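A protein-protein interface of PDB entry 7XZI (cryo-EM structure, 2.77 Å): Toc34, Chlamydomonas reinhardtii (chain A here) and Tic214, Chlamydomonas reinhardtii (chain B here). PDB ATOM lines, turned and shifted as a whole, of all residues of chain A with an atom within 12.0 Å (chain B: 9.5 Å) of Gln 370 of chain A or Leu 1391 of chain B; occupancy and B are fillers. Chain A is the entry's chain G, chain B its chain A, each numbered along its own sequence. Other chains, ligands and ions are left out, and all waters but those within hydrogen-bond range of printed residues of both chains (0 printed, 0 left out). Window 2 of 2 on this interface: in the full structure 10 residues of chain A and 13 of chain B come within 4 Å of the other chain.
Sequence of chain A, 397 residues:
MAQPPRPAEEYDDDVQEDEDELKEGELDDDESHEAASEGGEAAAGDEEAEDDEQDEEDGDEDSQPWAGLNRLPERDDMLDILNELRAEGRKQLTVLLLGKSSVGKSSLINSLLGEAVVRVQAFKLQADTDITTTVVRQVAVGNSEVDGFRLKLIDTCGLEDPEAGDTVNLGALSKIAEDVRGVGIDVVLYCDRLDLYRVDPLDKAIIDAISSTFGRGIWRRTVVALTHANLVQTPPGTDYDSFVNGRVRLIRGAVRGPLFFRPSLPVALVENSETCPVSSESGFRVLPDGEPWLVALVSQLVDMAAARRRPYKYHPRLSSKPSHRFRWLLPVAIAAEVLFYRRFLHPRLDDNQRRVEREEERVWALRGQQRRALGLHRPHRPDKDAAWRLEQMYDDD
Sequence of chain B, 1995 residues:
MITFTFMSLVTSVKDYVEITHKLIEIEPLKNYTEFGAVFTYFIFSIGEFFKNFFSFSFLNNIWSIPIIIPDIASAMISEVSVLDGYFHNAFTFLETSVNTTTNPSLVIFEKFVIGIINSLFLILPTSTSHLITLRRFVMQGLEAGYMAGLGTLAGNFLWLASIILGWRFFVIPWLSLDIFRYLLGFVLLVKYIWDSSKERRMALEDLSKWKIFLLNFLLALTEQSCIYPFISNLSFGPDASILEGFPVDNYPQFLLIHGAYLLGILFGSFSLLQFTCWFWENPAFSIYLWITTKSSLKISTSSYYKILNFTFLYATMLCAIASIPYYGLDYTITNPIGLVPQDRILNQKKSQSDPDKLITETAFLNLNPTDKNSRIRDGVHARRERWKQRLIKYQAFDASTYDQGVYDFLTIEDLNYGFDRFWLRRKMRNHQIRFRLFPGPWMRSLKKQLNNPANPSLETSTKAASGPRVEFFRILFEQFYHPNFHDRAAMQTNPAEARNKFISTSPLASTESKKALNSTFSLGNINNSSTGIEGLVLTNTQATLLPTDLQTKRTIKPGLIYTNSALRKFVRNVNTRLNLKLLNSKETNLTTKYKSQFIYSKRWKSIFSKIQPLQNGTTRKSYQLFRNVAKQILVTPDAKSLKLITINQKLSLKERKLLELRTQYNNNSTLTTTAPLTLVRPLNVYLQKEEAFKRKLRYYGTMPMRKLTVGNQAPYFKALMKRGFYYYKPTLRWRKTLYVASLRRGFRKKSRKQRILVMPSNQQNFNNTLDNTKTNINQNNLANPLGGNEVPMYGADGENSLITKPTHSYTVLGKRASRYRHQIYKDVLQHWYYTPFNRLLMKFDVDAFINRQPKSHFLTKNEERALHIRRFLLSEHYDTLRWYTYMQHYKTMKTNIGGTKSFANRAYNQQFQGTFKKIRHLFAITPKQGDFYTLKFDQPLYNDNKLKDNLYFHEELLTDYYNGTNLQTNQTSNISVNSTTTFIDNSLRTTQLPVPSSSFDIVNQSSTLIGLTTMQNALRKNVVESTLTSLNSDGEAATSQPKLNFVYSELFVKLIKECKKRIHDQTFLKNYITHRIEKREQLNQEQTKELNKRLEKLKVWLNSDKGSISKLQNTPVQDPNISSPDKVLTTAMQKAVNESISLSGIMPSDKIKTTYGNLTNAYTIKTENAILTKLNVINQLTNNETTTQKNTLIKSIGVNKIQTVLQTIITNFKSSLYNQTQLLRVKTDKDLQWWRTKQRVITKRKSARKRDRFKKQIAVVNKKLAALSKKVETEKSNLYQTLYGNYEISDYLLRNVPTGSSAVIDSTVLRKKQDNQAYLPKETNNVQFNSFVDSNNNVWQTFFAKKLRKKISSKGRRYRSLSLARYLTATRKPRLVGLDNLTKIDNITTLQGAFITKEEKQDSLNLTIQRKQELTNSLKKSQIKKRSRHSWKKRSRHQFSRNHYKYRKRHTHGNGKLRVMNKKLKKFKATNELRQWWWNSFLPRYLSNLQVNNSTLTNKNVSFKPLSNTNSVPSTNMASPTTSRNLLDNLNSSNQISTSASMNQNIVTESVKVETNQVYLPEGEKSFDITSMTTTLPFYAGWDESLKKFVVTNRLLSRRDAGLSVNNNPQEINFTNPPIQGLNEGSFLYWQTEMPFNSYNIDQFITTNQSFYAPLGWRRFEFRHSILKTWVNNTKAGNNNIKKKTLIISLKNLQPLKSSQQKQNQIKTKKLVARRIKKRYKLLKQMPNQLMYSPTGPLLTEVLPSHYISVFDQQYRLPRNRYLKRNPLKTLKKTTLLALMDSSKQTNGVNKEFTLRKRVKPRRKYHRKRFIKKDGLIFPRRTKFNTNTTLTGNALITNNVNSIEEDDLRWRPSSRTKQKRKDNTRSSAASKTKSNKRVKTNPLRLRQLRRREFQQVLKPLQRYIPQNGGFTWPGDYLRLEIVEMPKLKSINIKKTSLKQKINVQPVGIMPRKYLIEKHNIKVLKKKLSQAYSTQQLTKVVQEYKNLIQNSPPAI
CD1 of Leu 366 of chain A touches O of Asn 1381 of chain B (3.2 Å). Leu 366 of chain A touches Thr 1383 of chain B. Thr 1383 of chain B touches Arg 367 of chain A. Arg 367 of chain A touches Ile 1385 of chain B. O of Leu 1391 of chain B touches CA of Gln 370 of chain A (3.5 Å).
O of Thr 1383 of chain B sits at hydrogen-bond distance from N of Thr 1389 of chain B (3.1 Å).
Gln 370 of chain A touches one residue of chain B. Printed residues of chain A within 4 Å of Leu 1391 of chain B: Gln 370 (3.5 Å). No residue of chain B comes within 4 Å of Gly 368 of chain A. No residue of chain B comes within 4 Å of Ala 373 of chain A. Thr 1383 of chain B touches just these residues of chain A: Leu 366 and Arg 367. No residue of chain A comes within 4 Å of Gly 1393 of chain B. Of the printed residues of chain B, Leu 366 of chain A touches Asn 1381 (3.2 Å) and Thr 1383 (3.9 Å). Of the printed residues of chain A, Asn 1381 of chain B touches Leu 366. Arg 371 of chain A touches none of the printed residues of chain B. The nearest residue of chain A that does not touch Leu 1391 of chain B is Gln 369 of chain A (4.04 Å). The nearest printed residue of chain A that does not touch Asn 1381 of chain B is Arg 362 of chain A (6.3 Å).
Printed residues of chain A that touch a printed residue of chain B: Leu 366, Arg 367 and Gln 370. Hydrophobic or aromatic side chains of chain A within 4 Å of the printed part of chain B: Leu 366. Of the 16 printed residues of chain B, 4 touch a printed residue of chain A. Printed residues of chain B that touch a printed residue of chain A: Asn 1381, Thr 1383, Ile 1385 and Leu 1391. Hydrophobic or aromatic side chains of chain B that line the printed part of chain A: Ile 1385. Among the printed residues, 5 pairs touch across the chains.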
ATOM      1  N   GLU A 361       3.691 -12.870   1.317  1.00  0.00           N
ATOM      2  CA  GLU A 361       3.808 -14.222   0.783  1.00  0.00           C
ATOM      3  C   GLU A 361       5.080 -14.365  -0.036  1.00  0.00           C
ATOM      4  O   GLU A 361       5.821 -15.346   0.121  1.00  0.00           O
ATOM      5  CB  GLU A 361       2.581 -14.565  -0.061  1.00  0.00           C
ATOM      6  N   ARG A 362       5.379 -13.362  -0.869  1.00  0.00           N
ATOM      7  CA  ARG A 362       6.580 -13.413  -1.694  1.00  0.00           C
ATOM      8  C   ARG A 362       7.804 -13.710  -0.844  1.00  0.00           C
ATOM      9  O   ARG A 362       8.597 -14.601  -1.176  1.00  0.00           O
ATOM     10  CB  ARG A 362       6.757 -12.094  -2.447  1.00  0.00           C
ATOM     11  CG  ARG A 362       8.016 -12.024  -3.296  1.00  0.00           C
ATOM     12  CD  ARG A 362       8.239 -10.618  -3.836  1.00  0.00           C
ATOM     13  NE  ARG A 362       7.102 -10.141  -4.609  1.00  0.00           N
ATOM     14  N   VAL A 363       7.934 -13.020   0.294  1.00  0.00           N
ATOM     15  CA  VAL A 363       9.105 -13.211   1.143  1.00  0.00           C
ATOM     16  C   VAL A 363       9.245 -14.679   1.515  1.00  0.00           C
ATOM     17  O   VAL A 363      10.306 -15.288   1.327  1.00  0.00           O
ATOM     18  CB  VAL A 363       9.016 -12.317   2.393  1.00  0.00           C
ATOM     19  N   TRP A 364       8.149 -15.290   1.977  1.00  0.00           N
ATOM     20  CA  TRP A 364       8.219 -16.687   2.382  1.00  0.00           C
ATOM     21  C   TRP A 364       8.633 -17.573   1.220  1.00  0.00           C
ATOM     22  O   TRP A 364       9.442 -18.491   1.402  1.00  0.00           O
ATOM     23  CB  TRP A 364       6.883 -17.145   2.963  1.00  0.00           C
ATOM     24  CG  TRP A 364       6.689 -16.741   4.391  1.00  0.00           C
ATOM     25  CD1 TRP A 364       5.825 -15.799   4.868  1.00  0.00           C
ATOM     26  CD2 TRP A 364       7.385 -17.260   5.533  1.00  0.00           C
ATOM     27  NE1 TRP A 364       5.936 -15.704   6.234  1.00  0.00           N
ATOM     28  CE2 TRP A 364       6.887 -16.590   6.666  1.00  0.00           C
ATOM     29  CE3 TRP A 364       8.379 -18.229   5.704  1.00  0.00           C
ATOM     30  CZ2 TRP A 364       7.348 -16.856   7.955  1.00  0.00           C
ATOM     31  CZ3 TRP A 364       8.835 -18.492   6.984  1.00  0.00           C
ATOM     32  CH2 TRP A 364       8.320 -17.808   8.092  1.00  0.00           C
ATOM     33  N   ALA A 365       8.129 -17.285   0.016  1.00  0.00           N
ATOM     34  CA  ALA A 365       8.538 -18.058  -1.150  1.00  0.00           C
ATOM     35  C   ALA A 365      10.052 -18.048  -1.289  1.00  0.00           C
ATOM     36  O   ALA A 365      10.682 -19.101  -1.451  1.00  0.00           O
ATOM     37  CB  ALA A 365       7.872 -17.507  -2.410  1.00  0.00           C
ATOM     38  N   LEU A 366      10.659 -16.865  -1.165  1.00  0.00           N
ATOM     39  CA  LEU A 366      12.112 -16.779  -1.249  1.00  0.00           C
ATOM     40  C   LEU A 366      12.762 -17.600  -0.146  1.00  0.00           C
ATOM     41  O   LEU A 366      13.731 -18.330  -0.398  1.00  0.00           O
ATOM     42  CB  LEU A 366      12.551 -15.317  -1.186  1.00  0.00           C
ATOM     43  CG  LEU A 366      11.952 -14.440  -2.288  1.00  0.00           C
ATOM     44  CD1 LEU A 366      12.155 -12.967  -1.987  1.00  0.00           C
ATOM     45  CD2 LEU A 366      12.548 -14.797  -3.641  1.00  0.00           C
ATOM     46  N   ARG A 367      12.215 -17.528   1.071  1.00  0.00           N
ATOM     47  CA  ARG A 367      12.727 -18.357   2.155  1.00  0.00           C
ATOM     48  C   ARG A 367      12.683 -19.828   1.774  1.00  0.00           C
ATOM     49  O   ARG A 367      13.631 -20.576   2.046  1.00  0.00           O
ATOM     50  CB  ARG A 367      11.931 -18.106   3.435  1.00  0.00           C
ATOM     51  CG  ARG A 367      12.025 -16.684   3.960  1.00  0.00           C
ATOM     52  CD  ARG A 367      13.447 -16.329   4.369  1.00  0.00           C
ATOM     53  NE  ARG A 367      13.941 -17.189   5.437  1.00  0.00           N
ATOM     54  CZ  ARG A 367      13.752 -16.962   6.732  1.00  0.00           C
ATOM     55  NH1 ARG A 367      13.078 -15.907   7.159  1.00  0.00           N
ATOM     56  NH2 ARG A 367      14.253 -17.817   7.619  1.00  0.00           N
ATOM     57  N   GLY A 368      11.605 -20.253   1.107  1.00  0.00           N
ATOM     58  CA  GLY A 368      11.529 -21.631   0.659  1.00  0.00           C
ATOM     59  C   GLY A 368      12.701 -22.008  -0.224  1.00  0.00           C
ATOM     60  O   GLY A 368      13.297 -23.077  -0.059  1.00  0.00           O
ATOM     61  N   GLN A 369      13.079 -21.112  -1.140  1.00  0.00           N
ATOM     62  CA  GLN A 369      14.239 -21.373  -1.985  1.00  0.00           C
ATOM     63  C   GLN A 369      15.489 -21.567  -1.139  1.00  0.00           C
ATOM     64  O   GLN A 369      16.291 -22.471  -1.402  1.00  0.00           O
ATOM     65  CB  GLN A 369      14.434 -20.232  -2.982  1.00  0.00           C
ATOM     66  N   GLN A 370      15.650 -20.748  -0.095  1.00  0.00           N
ATOM     67  CA  GLN A 370      16.787 -20.915   0.802  1.00  0.00           C
ATOM     68  C   GLN A 370      16.764 -22.288   1.456  1.00  0.00           C
ATOM     69  O   GLN A 370      17.815 -22.908   1.658  1.00  0.00           O
ATOM     70  CB  GLN A 370      16.789 -19.812   1.859  1.00  0.00           C
ATOM     71  N   ARG A 371      15.572 -22.783   1.792  1.00  0.00           N
ATOM     72  CA  ARG A 371      15.473 -24.134   2.330  1.00  0.00           C
ATOM     73  C   ARG A 371      15.577 -25.174   1.223  1.00  0.00           C
ATOM     74  O   ARG A 371      15.995 -26.312   1.467  1.00  0.00           O
ATOM     75  CB  ARG A 371      14.175 -24.293   3.120  1.00  0.00           C
ATOM     76  CG  ARG A 371      14.091 -23.378   4.335  1.00  0.00           C
ATOM     77  CD  ARG A 371      15.404 -23.378   5.114  1.00  0.00           C
ATOM     78  NE  ARG A 371      15.385 -22.454   6.239  1.00  0.00           N
ATOM     79  CZ  ARG A 371      15.137 -22.806   7.495  1.00  0.00           C
ATOM     80  NH1 ARG A 371      14.889 -24.063   7.825  1.00  0.00           N
ATOM     81  NH2 ARG A 371      15.142 -21.874   8.443  1.00  0.00           N
ATOM     82  N   ARG A 372      15.192 -24.805  -0.003  1.00  0.00           N
ATOM     83  CA  ARG A 372      15.302 -25.741  -1.117  1.00  0.00           C
ATOM     84  C   ARG A 372      16.760 -26.067  -1.418  1.00  0.00           C
ATOM     85  O   ARG A 372      17.121 -27.238  -1.590  1.00  0.00           O
ATOM     86  CB  ARG A 372      14.612 -25.170  -2.355  1.00  0.00           C
ATOM     87  N   ALA A 373      17.610 -25.047  -1.482  1.00  0.00           N
ATOM     88  CA  ALA A 373      19.032 -25.271  -1.689  1.00  0.00           C
ATOM     89  C   ALA A 373      19.666 -25.863  -0.435  1.00  0.00           C
ATOM     90  O   ALA A 373      19.202 -25.630   0.685  1.00  0.00           O
ATOM     91  CB  ALA A 373      19.730 -23.965  -2.069  1.00  0.00           C
ATOM     92  N   LEU A 374      20.726 -26.647  -0.637  1.00  0.00           N
ATOM     93  CA  LEU A 374      21.502 -27.281   0.426  1.00  0.00           C
ATOM     94  C   LEU A 374      20.688 -28.270   1.252  1.00  0.00           C
ATOM     95  O   LEU A 374      21.117 -28.665   2.341  1.00  0.00           O
ATOM     96  CB  LEU A 374      22.146 -26.236   1.346  1.00  0.00           C
ATOM     97  N   GLY A 375      19.521 -28.677   0.763  1.00  0.00           N
ATOM     98  CA  GLY A 375      18.753 -29.718   1.438  1.00  0.00           C
ATOM     99  C   GLY A 375      18.324 -29.366   2.844  1.00  0.00           C
ATOM    100  O   GLY A 375      18.384 -30.215   3.743  1.00  0.00           O
ATOM    101  N   LEU A 376      17.890 -28.128   3.059  1.00  0.00           N
ATOM    102  CA  LEU A 376      17.430 -27.711   4.376  1.00  0.00           C
ATOM    103  C   LEU A 376      15.955 -28.049   4.560  1.00  0.00           C
ATOM    104  O   LEU A 376      15.179 -28.094   3.602  1.00  0.00           O
ATOM    105  CB  LEU A 376      17.654 -26.212   4.575  1.00  0.00           C
ATOM    106  N   HIS A 377      15.572 -28.288   5.812  1.00  0.00           N
ATOM    107  CA  HIS A 377      14.202 -28.661   6.118  1.00  0.00           C
ATOM    108  C   HIS A 377      13.297 -27.429   6.123  1.00  0.00           C
ATOM    109  O   HIS A 377      13.745 -26.289   5.970  1.00  0.00           O
ATOM    110  CB  HIS A 377      14.130 -29.392   7.458  1.00  0.00           C
ATOM    111  CG  HIS A 377      14.490 -28.540   8.636  1.00  0.00           C
ATOM    112  ND1 HIS A 377      13.572 -27.738   9.281  1.00  0.00           N
ATOM    113  CD2 HIS A 377      15.664 -28.365   9.286  1.00  0.00           C
ATOM    114  CE1 HIS A 377      14.166 -27.108  10.277  1.00  0.00           C
ATOM    115  NE2 HIS A 377      15.436 -27.469  10.301  1.00  0.00           N
ATOM    116  N   ARG A 378      11.999 -27.676   6.293  1.00  0.00           N
ATOM    117  CA  ARG A 378      11.017 -26.605   6.236  1.00  0.00           C
ATOM    118  C   ARG A 378      11.213 -25.629   7.396  1.00  0.00           C
ATOM    119  O   ARG A 378      11.586 -26.031   8.502  1.00  0.00           O
ATOM    120  CB  ARG A 378       9.602 -27.179   6.271  1.00  0.00           C
ATOM    121  N   PRO A 379      10.966 -24.338   7.169  1.00  0.00           N
ATOM    122  CA  PRO A 379      11.120 -23.341   8.234  1.00  0.00           C
ATOM    123  C   PRO A 379       9.937 -23.237   9.184  1.00  0.00           C
ATOM    124  O   PRO A 379       9.940 -22.346  10.038  1.00  0.00           O
ATOM    125  CB  PRO A 379      11.288 -22.036   7.440  1.00  0.00           C
ATOM    126  CG  PRO A 379      10.486 -22.260   6.209  1.00  0.00           C
ATOM    127  CD  PRO A 379      10.633 -23.721   5.873  1.00  0.00           C
ATOM    128  N   HIS A 380       8.946 -24.121   9.054  1.00  0.00           N
ATOM    129  CA  HIS A 380       7.768 -24.194   9.926  1.00  0.00           C
ATOM    130  C   HIS A 380       7.174 -22.809  10.198  1.00  0.00           C
ATOM    131  O   HIS A 380       7.142 -22.319  11.328  1.00  0.00           O
ATOM    132  CB  HIS A 380       8.085 -24.940  11.233  1.00  0.00           C
ATOM    133  CG  HIS A 380       9.215 -24.355  12.026  1.00  0.00           C
ATOM    134  ND1 HIS A 380      10.533 -24.697  11.807  1.00  0.00           N
ATOM    135  CD2 HIS A 380       9.223 -23.469  13.050  1.00  0.00           C
ATOM    136  CE1 HIS A 380      11.304 -24.036  12.653  1.00  0.00           C
ATOM    137  NE2 HIS A 380      10.534 -23.284  13.418  1.00  0.00           N
ATOM    138  N   ASP B1380      16.767  -5.722  -3.231  1.00  0.00           N
ATOM    139  CA  ASP B1380      16.415  -6.880  -4.049  1.00  0.00           C
ATOM    140  C   ASP B1380      15.654  -7.943  -3.263  1.00  0.00           C
ATOM    141  O   ASP B1380      15.201  -7.694  -2.141  1.00  0.00           O
ATOM    142  CB  ASP B1380      17.679  -7.498  -4.657  1.00  0.00           C
ATOM    143  N   ASN B1381      15.507  -9.132  -3.853  1.00  0.00           N
ATOM    144  CA  ASN B1381      14.786 -10.237  -3.228  1.00  0.00           C
ATOM    145  C   ASN B1381      15.538 -10.808  -2.031  1.00  0.00           C
ATOM    146  O   ASN B1381      15.100 -11.796  -1.432  1.00  0.00           O
ATOM    147  CB  ASN B1381      14.502 -11.343  -4.255  1.00  0.00           C
ATOM    148  CG  ASN B1381      15.763 -11.859  -4.932  1.00  0.00           C
ATOM    149  OD1 ASN B1381      16.713 -11.109  -5.160  1.00  0.00           O
ATOM    150  ND2 ASN B1381      15.771 -13.147  -5.261  1.00  0.00           N
ATOM    151  N   LEU B1382      16.664 -10.198  -1.675  1.00  0.00           N
ATOM    152  CA  LEU B1382      17.448 -10.646  -0.530  1.00  0.00           C
ATOM    153  C   LEU B1382      16.626 -10.523   0.748  1.00  0.00           C
ATOM    154  O   LEU B1382      16.250  -9.417   1.151  1.00  0.00           O
ATOM    155  CB  LEU B1382      18.728  -9.824  -0.424  1.00  0.00           C
ATOM    156  CG  LEU B1382      19.521  -9.710  -1.726  1.00  0.00           C
ATOM    157  CD1 LEU B1382      20.596  -8.643  -1.614  1.00  0.00           C
ATOM    158  CD2 LEU B1382      20.129 -11.054  -2.093  1.00  0.00           C
ATOM    159  N   THR B1383      16.346 -11.657   1.383  1.00  0.00           N
ATOM    160  CA  THR B1383      15.647 -11.651   2.656  1.00  0.00           C
ATOM    161  C   THR B1383      16.562 -11.121   3.756  1.00  0.00           C
ATOM    162  O   THR B1383      17.791 -11.199   3.669  1.00  0.00           O
ATOM    163  CB  THR B1383      15.158 -13.056   3.012  1.00  0.00           C
ATOM    164  OG1 THR B1383      16.282 -13.936   3.139  1.00  0.00           O
ATOM    165  CG2 THR B1383      14.230 -13.585   1.929  1.00  0.00           C
ATOM    166  N   LYS B1384      15.948 -10.571   4.805  1.00  0.00           N
ATOM    167  CA  LYS B1384      16.716  -9.955   5.886  1.00  0.00           C
ATOM    168  C   LYS B1384      15.991 -10.201   7.206  1.00  0.00           C
ATOM    169  O   LYS B1384      15.099  -9.435   7.580  1.00  0.00           O
ATOM    170  CB  LYS B1384      16.919  -8.467   5.636  1.00  0.00           C
ATOM    171  N   ILE B1385      16.379 -11.268   7.898  1.00  0.00           N
ATOM    172  CA  ILE B1385      16.020 -11.495   9.292  1.00  0.00           C
ATOM    173  C   ILE B1385      17.324 -11.630  10.067  1.00  0.00           C
ATOM    174  O   ILE B1385      18.106 -12.555   9.814  1.00  0.00           O
ATOM    175  CB  ILE B1385      15.126 -12.733   9.470  1.00  0.00           C
ATOM    176  CG1 ILE B1385      15.095 -13.169  10.937  1.00  0.00           C
ATOM    177  CG2 ILE B1385      15.581 -13.870   8.559  1.00  0.00           C
ATOM    178  N   ILE B1388      21.532 -10.722   6.960  1.00  0.00           N
ATOM    179  CA  ILE B1388      20.936 -10.769   5.631  1.00  0.00           C
ATOM    180  C   ILE B1388      21.340 -12.059   4.929  1.00  0.00           C
ATOM    181  O   ILE B1388      22.515 -12.451   4.932  1.00  0.00           O
ATOM    182  CB  ILE B1388      21.349  -9.534   4.813  1.00  0.00           C
ATOM    183  CG1 ILE B1388      20.869  -8.256   5.503  1.00  0.00           C
ATOM    184  CG2 ILE B1388      20.794  -9.614   3.399  1.00  0.00           C
ATOM    185  CD1 ILE B1388      21.189  -6.990   4.738  1.00  0.00           C
ATOM    186  N   THR B1389      20.363 -12.727   4.320  1.00  0.00           N
ATOM    187  CA  THR B1389      20.577 -13.984   3.620  1.00  0.00           C
ATOM    188  C   THR B1389      20.191 -13.829   2.156  1.00  0.00           C
ATOM    189  O   THR B1389      19.149 -13.249   1.838  1.00  0.00           O
ATOM    190  CB  THR B1389      19.762 -15.119   4.257  1.00  0.00           C
ATOM    191  OG1 THR B1389      20.018 -15.162   5.666  1.00  0.00           O
ATOM    192  CG2 THR B1389      20.135 -16.460   3.642  1.00  0.00           C
ATOM    193  N   THR B1390      21.037 -14.345   1.269  1.00  0.00           N
ATOM    194  CA  THR B1390      20.799 -14.275  -0.165  1.00  0.00           C
ATOM    195  C   THR B1390      19.855 -15.403  -0.580  1.00  0.00           C
ATOM    196  O   THR B1390      19.224 -16.055   0.257  1.00  0.00           O
ATOM    197  CB  THR B1390      22.122 -14.324  -0.926  1.00  0.00           C
ATOM    198  OG1 THR B1390      21.872 -14.195  -2.331  1.00  0.00           O
ATOM    199  CG2 THR B1390      22.841 -15.638  -0.665  1.00  0.00           C
ATOM    200  N   LEU B1391      19.741 -15.638  -1.891  1.00  0.00           N
ATOM    201  CA  LEU B1391      18.880 -16.714  -2.375  1.00  0.00           C
ATOM    202  C   LEU B1391      19.342 -18.071  -1.865  1.00  0.00           C
ATOM    203  O   LEU B1391      18.512 -18.922  -1.522  1.00  0.00           O
ATOM    204  CB  LEU B1391      18.837 -16.707  -3.905  1.00  0.00           C
ATOM    205  N   GLN B1392      20.651 -18.295  -1.814  1.00  0.00           N
ATOM    206  CA  GLN B1392      21.205 -19.516  -1.251  1.00  0.00           C
ATOM    207  C   GLN B1392      21.192 -19.447   0.274  1.00  0.00           C
ATOM    208  O   GLN B1392      20.804 -18.444   0.877  1.00  0.00           O
ATOM    209  CB  GLN B1392      22.624 -19.747  -1.771  1.00  0.00           C
ATOM    210  N   GLY B1393      21.625 -20.541   0.903  1.00  0.00           N
ATOM    211  CA  GLY B1393      21.633 -20.602   2.354  1.00  0.00           C
ATOM    212  C   GLY B1393      22.693 -19.741   3.006  1.00  0.00           C
ATOM    213  O   GLY B1393      22.586 -19.443   4.200  1.00  0.00           O
ATOM    214  N   ALA B1394      23.711 -19.334   2.254  1.00  0.00           N
ATOM    215  CA  ALA B1394      24.800 -18.548   2.808  1.00  0.00           C
ATOM    216  C   ALA B1394      24.377 -17.102   3.033  1.00  0.00           C
ATOM    217  O   ALA B1394      23.515 -16.567   2.329  1.00  0.00           O
ATOM    218  CB  ALA B1394      26.019 -18.594   1.887  1.00  0.00           C
ATOM    219  N   PHE B1395      24.991 -16.472   4.030  1.00  0.00           N
ATOM    220  CA  PHE B1395      24.764 -15.056   4.275  1.00  0.00           C
ATOM    221  C   PHE B1395      25.456 -14.215   3.210  1.00  0.00           C
ATOM    222  O   PHE B1395      26.440 -14.634   2.595  1.00  0.00           O
ATOM    223  CB  PHE B1395      25.270 -14.663   5.664  1.00  0.00           C
ATOM    224  CG  PHE B1395      24.452 -15.229   6.789  1.00  0.00           C
ATOM    225  CD1 PHE B1395      23.115 -15.534   6.603  1.00  0.00           C
ATOM    226  CD2 PHE B1395      25.021 -15.458   8.031  1.00  0.00           C
ATOM    227  CE1 PHE B1395      22.358 -16.056   7.634  1.00  0.00           C
ATOM    228  CE2 PHE B1395      24.268 -15.979   9.067  1.00  0.00           C
ATOM    229  CZ  PHE B1395      22.936 -16.278   8.867  1.00  0.00           C
ATOM    230  N   ILE B1396      24.922 -13.013   2.988  1.00  0.00           N
ATOM    231  CA  ILE B1396      25.487 -12.121   1.984  1.00  0.00           C
ATOM    232  C   ILE B1396      26.859 -11.634   2.441  1.00  0.00           C
ATOM    233  O   ILE B1396      27.112 -11.438   3.638  1.00  0.00           O
ATOM    234  CB  ILE B1396      24.528 -10.949   1.703  1.00  0.00           C
ATOM    235  CG1 ILE B1396      24.929 -10.214   0.424  1.00  0.00           C
ATOM    236  CG2 ILE B1396      24.479  -9.987   2.882  1.00  0.00           C
ATOM    237  CD1 ILE B1396      23.880  -9.252  -0.082  1.00  0.00           C
ATOM    238  N   GLU B1400      29.254  -8.892  -2.103  1.00  0.00           N
ATOM    239  CA  GLU B1400      27.953  -9.192  -2.694  1.00  0.00           C
ATOM    240  C   GLU B1400      26.977  -8.039  -2.502  1.00  0.00           C
ATOM    241  O   GLU B1400      26.143  -7.772  -3.374  1.00  0.00           O
ATOM    242  CB  GLU B1400      27.391 -10.481  -2.099  1.00  0.00           C
